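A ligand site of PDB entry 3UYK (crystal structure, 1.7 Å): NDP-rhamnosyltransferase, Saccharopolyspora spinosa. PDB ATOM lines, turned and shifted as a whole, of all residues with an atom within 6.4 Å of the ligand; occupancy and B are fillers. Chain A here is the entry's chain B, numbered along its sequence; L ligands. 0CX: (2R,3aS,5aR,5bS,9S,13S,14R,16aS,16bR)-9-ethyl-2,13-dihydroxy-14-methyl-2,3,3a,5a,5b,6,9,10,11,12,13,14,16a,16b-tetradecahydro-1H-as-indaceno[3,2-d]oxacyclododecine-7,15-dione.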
ATOM      1  N   LEU A   9     -14.922   3.705  -6.874  1.00  0.00           N
ATOM      2  CA  LEU A   9     -15.213   4.722  -7.858  1.00  0.00           C
ATOM      3  C   LEU A   9     -15.206   4.126  -9.277  1.00  0.00           C
ATOM      4  O   LEU A   9     -14.521   3.167  -9.509  1.00  0.00           O
ATOM      5  CB  LEU A   9     -14.079   5.744  -7.828  1.00  0.00           C
ATOM      6  CG  LEU A   9     -14.230   6.871  -6.855  1.00  0.00           C
ATOM      7  CD1 LEU A   9     -13.144   7.902  -7.188  1.00  0.00           C
ATOM      8  CD2 LEU A   9     -15.590   7.526  -6.878  1.00  0.00           C
ATOM      9  N   PRO A  10     -15.931   4.716 -10.253  1.00  0.00           N
ATOM     10  CA  PRO A  10     -16.045   4.023 -11.544  1.00  0.00           C
ATOM     11  C   PRO A  10     -14.868   4.198 -12.473  1.00  0.00           C
ATOM     12  O   PRO A  10     -15.030   4.574 -13.636  1.00  0.00           O
ATOM     13  CB  PRO A  10     -17.306   4.642 -12.180  1.00  0.00           C
ATOM     14  CG  PRO A  10     -17.333   6.000 -11.606  1.00  0.00           C
ATOM     15  CD  PRO A  10     -16.856   5.850 -10.175  1.00  0.00           C
ATOM     16  N   TYR A  11     -13.666   3.922 -11.945  1.00  0.00           N
ATOM     17  CA  TYR A  11     -12.425   4.008 -12.703  1.00  0.00           C
ATOM     18  C   TYR A  11     -11.645   2.723 -12.455  1.00  0.00           C
ATOM     19  O   TYR A  11     -11.440   2.347 -11.275  1.00  0.00           O
ATOM     20  CB  TYR A  11     -11.588   5.188 -12.274  1.00  0.00           C
ATOM     21  CG  TYR A  11     -12.410   6.455 -12.442  1.00  0.00           C
ATOM     22  CD1 TYR A  11     -12.618   6.964 -13.726  1.00  0.00           C
ATOM     23  CD2 TYR A  11     -13.088   7.031 -11.384  1.00  0.00           C
ATOM     24  CE1 TYR A  11     -13.420   8.070 -13.940  1.00  0.00           C
ATOM     25  CE2 TYR A  11     -13.899   8.142 -11.568  1.00  0.00           C
ATOM     26  CZ  TYR A  11     -14.051   8.662 -12.850  1.00  0.00           C
ATOM     27  OH  TYR A  11     -14.857   9.751 -13.080  1.00  0.00           O
ATOM     28  N   THR A  13      -8.587   1.863 -12.548  1.00  0.00           N
ATOM     29  CA  THR A  13      -7.453   1.863 -11.645  1.00  0.00           C
ATOM     30  C   THR A  13      -7.774   1.852 -10.111  1.00  0.00           C
ATOM     31  O   THR A  13      -7.019   1.342  -9.244  1.00  0.00           O
ATOM     32  CB  THR A  13      -6.536   3.053 -11.995  1.00  0.00           C
ATOM     33  OG1 THR A  13      -5.550   3.155 -10.969  1.00  0.00           O
ATOM     34  CG2 THR A  13      -7.328   4.236 -11.900  1.00  0.00           C
ATOM     35  N   HIS A  14      -8.892   2.463  -9.720  1.00  0.00           N
ATOM     36  CA  HIS A  14      -9.352   2.376  -8.323  1.00  0.00           C
ATOM     37  C   HIS A  14      -9.771   0.967  -7.912  1.00  0.00           C
ATOM     38  O   HIS A  14      -9.465   0.534  -6.826  1.00  0.00           O
ATOM     39  CB  HIS A  14     -10.544   3.321  -8.170  1.00  0.00           C
ATOM     40  CG  HIS A  14     -10.118   4.783  -8.206  1.00  0.00           C
ATOM     41  ND1 HIS A  14     -10.214   5.584  -7.122  1.00  0.00           N
ATOM     42  CD2 HIS A  14      -9.565   5.559  -9.230  1.00  0.00           C
ATOM     43  CE1 HIS A  14      -9.731   6.809  -7.442  1.00  0.00           C
ATOM     44  NE2 HIS A  14      -9.349   6.800  -8.728  1.00  0.00           N
ATOM     45  N   TRP A  88     -11.059  20.398  -5.220  1.00  0.00           N
ATOM     46  CA  TRP A  88     -11.376  19.275  -4.417  1.00  0.00           C
ATOM     47  C   TRP A  88     -12.798  19.372  -3.886  1.00  0.00           C
ATOM     48  O   TRP A  88     -13.461  18.313  -3.730  1.00  0.00           O
ATOM     49  CB  TRP A  88     -10.363  19.222  -3.229  1.00  0.00           C
ATOM     50  CG  TRP A  88      -9.043  18.634  -3.750  1.00  0.00           C
ATOM     51  CD1 TRP A  88      -7.854  19.307  -4.140  1.00  0.00           C
ATOM     52  CD2 TRP A  88      -8.770  17.217  -3.979  1.00  0.00           C
ATOM     53  NE1 TRP A  88      -6.923  18.376  -4.542  1.00  0.00           N
ATOM     54  CE2 TRP A  88      -7.400  17.124  -4.464  1.00  0.00           C
ATOM     55  CE3 TRP A  88      -9.503  16.027  -3.751  1.00  0.00           C
ATOM     56  CZ2 TRP A  88      -6.772  15.883  -4.729  1.00  0.00           C
ATOM     57  CZ3 TRP A  88      -8.906  14.774  -4.081  1.00  0.00           C
ATOM     58  CH2 TRP A  88      -7.544  14.691  -4.593  1.00  0.00           C
ATOM     59  N   GLN A  90     -15.238  20.688  -5.713  1.00  0.00           N
ATOM     60  CA  GLN A  90     -16.042  20.312  -6.869  1.00  0.00           C
ATOM     61  C   GLN A  90     -16.061  18.798  -7.068  1.00  0.00           C
ATOM     62  O   GLN A  90     -17.102  18.189  -7.451  1.00  0.00           O
ATOM     63  CB  GLN A  90     -15.527  21.019  -8.087  1.00  0.00           C
ATOM     64  CG  GLN A  90     -16.392  20.752  -9.355  1.00  0.00           C
ATOM     65  CD  GLN A  90     -17.829  21.260  -9.189  1.00  0.00           C
ATOM     66  OE1 GLN A  90     -18.788  20.467  -9.158  1.00  0.00           O
ATOM     67  NE2 GLN A  90     -17.984  22.565  -9.026  1.00  0.00           N
ATOM     68  N   THR A  91     -14.917  18.140  -6.816  1.00  0.00           N
ATOM     69  CA  THR A  91     -14.834  16.678  -6.916  1.00  0.00           C
ATOM     70  C   THR A  91     -15.816  16.057  -5.882  1.00  0.00           C
ATOM     71  O   THR A  91     -16.605  15.125  -6.209  1.00  0.00           O
ATOM     72  CB  THR A  91     -13.420  16.236  -6.551  1.00  0.00           C
ATOM     73  OG1 THR A  91     -12.480  16.896  -7.420  1.00  0.00           O
ATOM     74  CG2 THR A  91     -13.233  14.699  -6.715  1.00  0.00           C
ATOM     75  N   ALA A  92     -15.833  16.549  -4.627  1.00  0.00           N
ATOM     76  CA  ALA A  92     -16.768  16.022  -3.630  1.00  0.00           C
ATOM     77  C   ALA A  92     -18.206  16.275  -4.067  1.00  0.00           C
ATOM     78  O   ALA A  92     -19.039  15.403  -3.851  1.00  0.00           O
ATOM     79  CB  ALA A  92     -16.556  16.731  -2.312  1.00  0.00           C
ATOM     80  N   ASN A  94     -19.386  16.478  -7.090  1.00  0.00           N
ATOM     81  CA  ASN A  94     -19.672  15.532  -8.177  1.00  0.00           C
ATOM     82  C   ASN A  94     -20.044  14.150  -7.629  1.00  0.00           C
ATOM     83  O   ASN A  94     -21.051  13.523  -8.065  1.00  0.00           O
ATOM     84  CB  ASN A  94     -18.486  15.425  -9.153  1.00  0.00           C
ATOM     85  CG  ASN A  94     -18.258  16.667  -9.953  1.00  0.00           C
ATOM     86  OD1 ASN A  94     -19.088  17.528 -10.004  1.00  0.00           O
ATOM     87  ND2 ASN A  94     -17.063  16.752 -10.629  1.00  0.00           N
ATOM     88  N   VAL A  95     -19.221  13.655  -6.727  1.00  0.00           N
ATOM     89  CA  VAL A  95     -19.396  12.365  -6.163  1.00  0.00           C
ATOM     90  C   VAL A  95     -20.657  12.325  -5.284  1.00  0.00           C
ATOM     91  O   VAL A  95     -21.411  11.317  -5.318  1.00  0.00           O
ATOM     92  CB  VAL A  95     -18.143  11.933  -5.348  1.00  0.00           C
ATOM     93  CG1 VAL A  95     -18.293  10.502  -4.872  1.00  0.00           C
ATOM     94  CG2 VAL A  95     -16.977  11.786  -6.331  1.00  0.00           C
ATOM     95  N   SER A  98     -23.767  12.335  -7.685  1.00  0.00           N
ATOM     96  CA  SER A  98     -23.847  10.958  -8.175  1.00  0.00           C
ATOM     97  C   SER A  98     -24.290   9.913  -7.093  1.00  0.00           C
ATOM     98  O   SER A  98     -25.096   8.953  -7.387  1.00  0.00           O
ATOM     99  CB  SER A  98     -22.507  10.611  -8.847  1.00  0.00           C
ATOM    100  OG  SER A  98     -22.492   9.290  -9.273  1.00  0.00           O
ATOM    101  N   GLN A 102     -27.856   7.647  -7.389  1.00  0.00           N
ATOM    102  CA  GLN A 102     -27.797   6.199  -7.498  1.00  0.00           C
ATOM    103  C   GLN A 102     -28.118   5.457  -6.262  1.00  0.00           C
ATOM    104  O   GLN A 102     -28.114   4.231  -6.269  1.00  0.00           O
ATOM    105  CB  GLN A 102     -26.396   5.788  -8.045  1.00  0.00           C
ATOM    106  CG  GLN A 102     -26.077   6.413  -9.394  1.00  0.00           C
ATOM    107  CD  GLN A 102     -24.693   6.007  -9.923  1.00  0.00           C
ATOM    108  OE1 GLN A 102     -23.719   6.731  -9.755  1.00  0.00           O
ATOM    109  NE2 GLN A 102     -24.610   4.842 -10.533  1.00  0.00           N
ATOM    110  N   ASP A 121     -14.076   2.468  -1.721  1.00  0.00           N
ATOM    111  CA  ASP A 121     -12.969   3.333  -2.109  1.00  0.00           C
ATOM    112  C   ASP A 121     -13.102   4.649  -1.298  1.00  0.00           C
ATOM    113  O   ASP A 121     -14.221   5.153  -1.134  1.00  0.00           O
ATOM    114  CB  ASP A 121     -13.220   3.603  -3.644  1.00  0.00           C
ATOM    115  CG  ASP A 121     -12.214   4.537  -4.264  1.00  0.00           C
ATOM    116  OD1 ASP A 121     -11.910   5.627  -3.749  1.00  0.00           O
ATOM    117  OD2 ASP A 121     -11.616   4.095  -5.261  1.00  0.00           O
ATOM    118  N   CYS A 123     -12.877   7.615  -1.898  1.00  0.00           N
ATOM    119  CA  CYS A 123     -13.594   8.661  -2.605  1.00  0.00           C
ATOM    120  C   CYS A 123     -15.075   8.326  -2.956  1.00  0.00           C
ATOM    121  O   CYS A 123     -15.780   9.237  -3.401  1.00  0.00           O
ATOM    122  CB  CYS A 123     -12.887   9.064  -3.838  1.00  0.00           C
ATOM    123  SG  CYS A 123     -11.420  10.120  -3.351  1.00  0.00           S
ATOM    124  N   TRP A 143      -6.191   4.175  -2.250  1.00  0.00           N
ATOM    125  CA  TRP A 143      -5.465   3.541  -3.331  1.00  0.00           C
ATOM    126  C   TRP A 143      -4.016   3.944  -3.324  1.00  0.00           C
ATOM    127  O   TRP A 143      -3.149   3.367  -3.993  1.00  0.00           O
ATOM    128  CB  TRP A 143      -6.139   3.872  -4.670  1.00  0.00           C
ATOM    129  CG  TRP A 143      -5.926   5.315  -4.945  1.00  0.00           C
ATOM    130  CD1 TRP A 143      -4.764   5.959  -5.403  1.00  0.00           C
ATOM    131  CD2 TRP A 143      -6.879   6.344  -4.679  1.00  0.00           C
ATOM    132  NE1 TRP A 143      -4.962   7.335  -5.455  1.00  0.00           N
ATOM    133  CE2 TRP A 143      -6.219   7.622  -4.990  1.00  0.00           C
ATOM    134  CE3 TRP A 143      -8.154   6.349  -4.131  1.00  0.00           C
ATOM    135  CZ2 TRP A 143      -6.866   8.825  -4.830  1.00  0.00           C
ATOM    136  CZ3 TRP A 143      -8.792   7.583  -3.975  1.00  0.00           C
ATOM    137  CH2 TRP A 143      -8.167   8.788  -4.312  1.00  0.00           C
ATOM    138  N   PHE A 152     -12.211  18.298   0.210  1.00  0.00           N
ATOM    139  CA  PHE A 152     -13.088  17.170  -0.193  1.00  0.00           C
ATOM    140  C   PHE A 152     -13.961  16.701   0.984  1.00  0.00           C
ATOM    141  O   PHE A 152     -15.202  16.673   0.898  1.00  0.00           O
ATOM    142  CB  PHE A 152     -12.242  16.048  -0.795  1.00  0.00           C
ATOM    143  CG  PHE A 152     -13.063  14.899  -1.248  1.00  0.00           C
ATOM    144  CD1 PHE A 152     -13.397  13.912  -0.322  1.00  0.00           C
ATOM    145  CD2 PHE A 152     -13.441  14.768  -2.606  1.00  0.00           C
ATOM    146  CE1 PHE A 152     -14.163  12.802  -0.697  1.00  0.00           C
ATOM    147  CE2 PHE A 152     -14.256  13.683  -2.977  1.00  0.00           C
ATOM    148  CZ  PHE A 152     -14.623  12.743  -1.988  1.00  0.00           C
ATOM    149  N   MET A 228      -6.310   6.155 -18.756  1.00  0.00           N
ATOM    150  CA  MET A 228      -7.078   7.208 -18.147  1.00  0.00           C
ATOM    151  C   MET A 228      -6.374   8.549 -18.193  1.00  0.00           C
ATOM    152  O   MET A 228      -6.991   9.578 -18.526  1.00  0.00           O
ATOM    153  CB  MET A 228      -7.417   6.879 -16.702  1.00  0.00           C
ATOM    154  CG  MET A 228      -8.344   7.893 -16.061  1.00  0.00           C
ATOM    155  SD  MET A 228      -8.683   7.377 -14.344  1.00  0.00           S
ATOM    156  CE  MET A 228      -7.166   7.879 -13.489  1.00  0.00           C
ATOM    157  N   TYR A 315      -3.042  15.444 -12.368  1.00  0.00           N
ATOM    158  CA  TYR A 315      -4.301  15.802 -11.603  1.00  0.00           C
ATOM    159  C   TYR A 315      -4.399  15.047 -10.267  1.00  0.00           C
ATOM    160  O   TYR A 315      -3.559  14.170  -9.953  1.00  0.00           O
ATOM    161  CB  TYR A 315      -5.553  15.493 -12.491  1.00  0.00           C
ATOM    162  CG  TYR A 315      -5.535  14.121 -13.125  1.00  0.00           C
ATOM    163  CD1 TYR A 315      -5.376  12.933 -12.379  1.00  0.00           C
ATOM    164  CD2 TYR A 315      -5.588  13.989 -14.498  1.00  0.00           C
ATOM    165  CE1 TYR A 315      -5.394  11.654 -12.939  1.00  0.00           C
ATOM    166  CE2 TYR A 315      -5.568  12.734 -15.053  1.00  0.00           C
ATOM    167  CZ  TYR A 315      -5.446  11.583 -14.283  1.00  0.00           C
ATOM    168  OH  TYR A 315      -5.450  10.352 -14.930  1.00  0.00           O
ATOM    169  N   PHE A 316      -5.438  15.426  -9.495  1.00  0.00           N
ATOM    170  CA  PHE A 316      -5.773  14.742  -8.232  1.00  0.00           C
ATOM    171  C   PHE A 316      -4.538  14.536  -7.367  1.00  0.00           C
ATOM    172  O   PHE A 316      -3.853  15.528  -7.091  1.00  0.00           O
ATOM    173  CB  PHE A 316      -6.598  13.485  -8.526  1.00  0.00           C
ATOM    174  CG  PHE A 316      -7.899  13.866  -9.114  1.00  0.00           C
ATOM    175  CD1 PHE A 316      -8.119  13.709 -10.506  1.00  0.00           C
ATOM    176  CD2 PHE A 316      -8.886  14.515  -8.315  1.00  0.00           C
ATOM    177  CE1 PHE A 316      -9.348  14.161 -11.073  1.00  0.00           C
ATOM    178  CE2 PHE A 316     -10.117  14.905  -8.876  1.00  0.00           C
ATOM    179  CZ  PHE A 316     -10.314  14.774 -10.256  1.00  0.00           C
ATOM    180  N   ASP A 317      -4.245  13.283  -6.994  1.00  0.00           N
ATOM    181  CA  ASP A 317      -3.189  13.011  -5.999  1.00  0.00           C
ATOM    182  C   ASP A 317      -1.778  13.009  -6.542  1.00  0.00           C
ATOM    183  O   ASP A 317      -0.839  12.750  -5.822  1.00  0.00           O
ATOM    184  CB  ASP A 317      -3.491  11.686  -5.292  1.00  0.00           C
ATOM    185  CG  ASP A 317      -3.686  10.596  -6.269  1.00  0.00           C
ATOM    186  OD1 ASP A 317      -4.579  10.725  -7.178  1.00  0.00           O
ATOM    187  OD2 ASP A 317      -3.005   9.628  -6.066  1.00  0.00           O
HETATM  188  O4  0CX L   1     -14.521  14.758 -10.647  1.00  0.00           O
HETATM  189  C15 0CX L   1     -14.234  13.675 -11.181  1.00  0.00           C
HETATM  190  C16 0CX L   1     -14.498  13.531 -12.629  1.00  0.00           C
HETATM  191  C24 0CX L   1     -13.329  14.153 -13.419  1.00  0.00           C
HETATM  192  C17 0CX L   1     -15.794  14.241 -12.979  1.00  0.00           C
HETATM  193  O5  0CX L   1     -15.923  13.919 -14.352  1.00  0.00           O
HETATM  194  C18 0CX L   1     -17.059  13.817 -12.236  1.00  0.00           C
HETATM  195  C19 0CX L   1     -17.794  12.670 -12.900  1.00  0.00           C
HETATM  196  C20 0CX L   1     -18.621  11.863 -11.918  1.00  0.00           C
HETATM  197  C21 0CX L   1     -17.734  10.956 -11.087  1.00  0.00           C
HETATM  198  C22 0CX L   1     -18.562   9.741 -10.660  1.00  0.00           C
HETATM  199  C23 0CX L   1     -18.017   8.935  -9.498  1.00  0.00           C
HETATM  200  O1  0CX L   1     -17.236  11.821 -10.037  1.00  0.00           O
HETATM  201  C14 0CX L   1     -13.639  12.526 -10.509  1.00  0.00           C
HETATM  202  C13 0CX L   1     -12.819  11.558 -11.062  1.00  0.00           C
HETATM  203  C12 0CX L   1     -12.196  10.669  -9.974  1.00  0.00           C
HETATM  204  C11 0CX L   1     -10.720  10.936  -9.746  1.00  0.00           C
HETATM  205  C10 0CX L   1      -9.707  10.373 -10.758  1.00  0.00           C
HETATM  206  C9  0CX L   1      -8.417  10.174  -9.868  1.00  0.00           C
HETATM  207  C8  0CX L   1      -8.784  10.434  -8.395  1.00  0.00           C
HETATM  208  O2  0CX L   1      -7.831   8.871  -9.999  1.00  0.00           O
HETATM  209  C7  0CX L   1     -10.295  10.308  -8.414  1.00  0.00           C
HETATM  210  C6  0CX L   1     -11.016  10.899  -7.225  1.00  0.00           C
HETATM  211  C5  0CX L   1     -12.306  11.201  -7.399  1.00  0.00           C
HETATM  212  C4  0CX L   1     -13.034  11.008  -8.717  1.00  0.00           C
HETATM  213  C3  0CX L   1     -13.778  12.310  -9.058  1.00  0.00           C
HETATM  214  C2  0CX L   1     -15.222  12.312  -8.618  1.00  0.00           C
HETATM  215  C1  0CX L   1     -15.984  11.413  -9.553  1.00  0.00           C
HETATM  216  O3  0CX L   1     -15.582  10.342  -9.924  1.00  0.00           O
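Merely in contact with the ligand: Val 95 (2.9 Å), Pro 10 (3.4 Å), Thr 91 (3.4 Å), Leu 9 (3.4 Å), Phe 316 (3.6 Å), Met 228 (3.7 Å) and Cys 123 (3.97 Å).
Hydrophobic or aromatic side chains that line the ligand: Leu 9, Pro 10, Tyr 11, His 14, Val 95, Met 228 and Phe 316.
Ten residues have an atom within 4 Å of the ligand: Leu 9, Pro 10, Tyr 11, His 14, Thr 91, Asn 94, Val 95, Cys 123, Met 228 and Phe 316.
The nearest printed residue that does not touch the ligand is Ser 98 (4.2 Å).
A ring nitrogen (ND1) of His 14 lies within hydrogen-bond range of the side-chain carboxylate of Asp 121, at 2.8 Å.
The side-chain amide oxygen (OD1) of Asn 94 sits close to the side-chain amide oxygen (OE1) of Gln 90 (3.1 Å).
The backbone NH of Cys 123 lies within hydrogen-bond range of the side-chain carboxylate of Asp 121.
A ring nitrogen (NE2) of His 14 is in hydrogen-bond range of an oxygen (O2) of the ligand (2.9 Å).
O3 of the ligand lies close to OH of Tyr 11 (3.3 Å).
The side-chain amide nitrogen of Asn 94 is in hydrogen-bond range of an oxygen (O4) of the ligand (3.2 Å).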
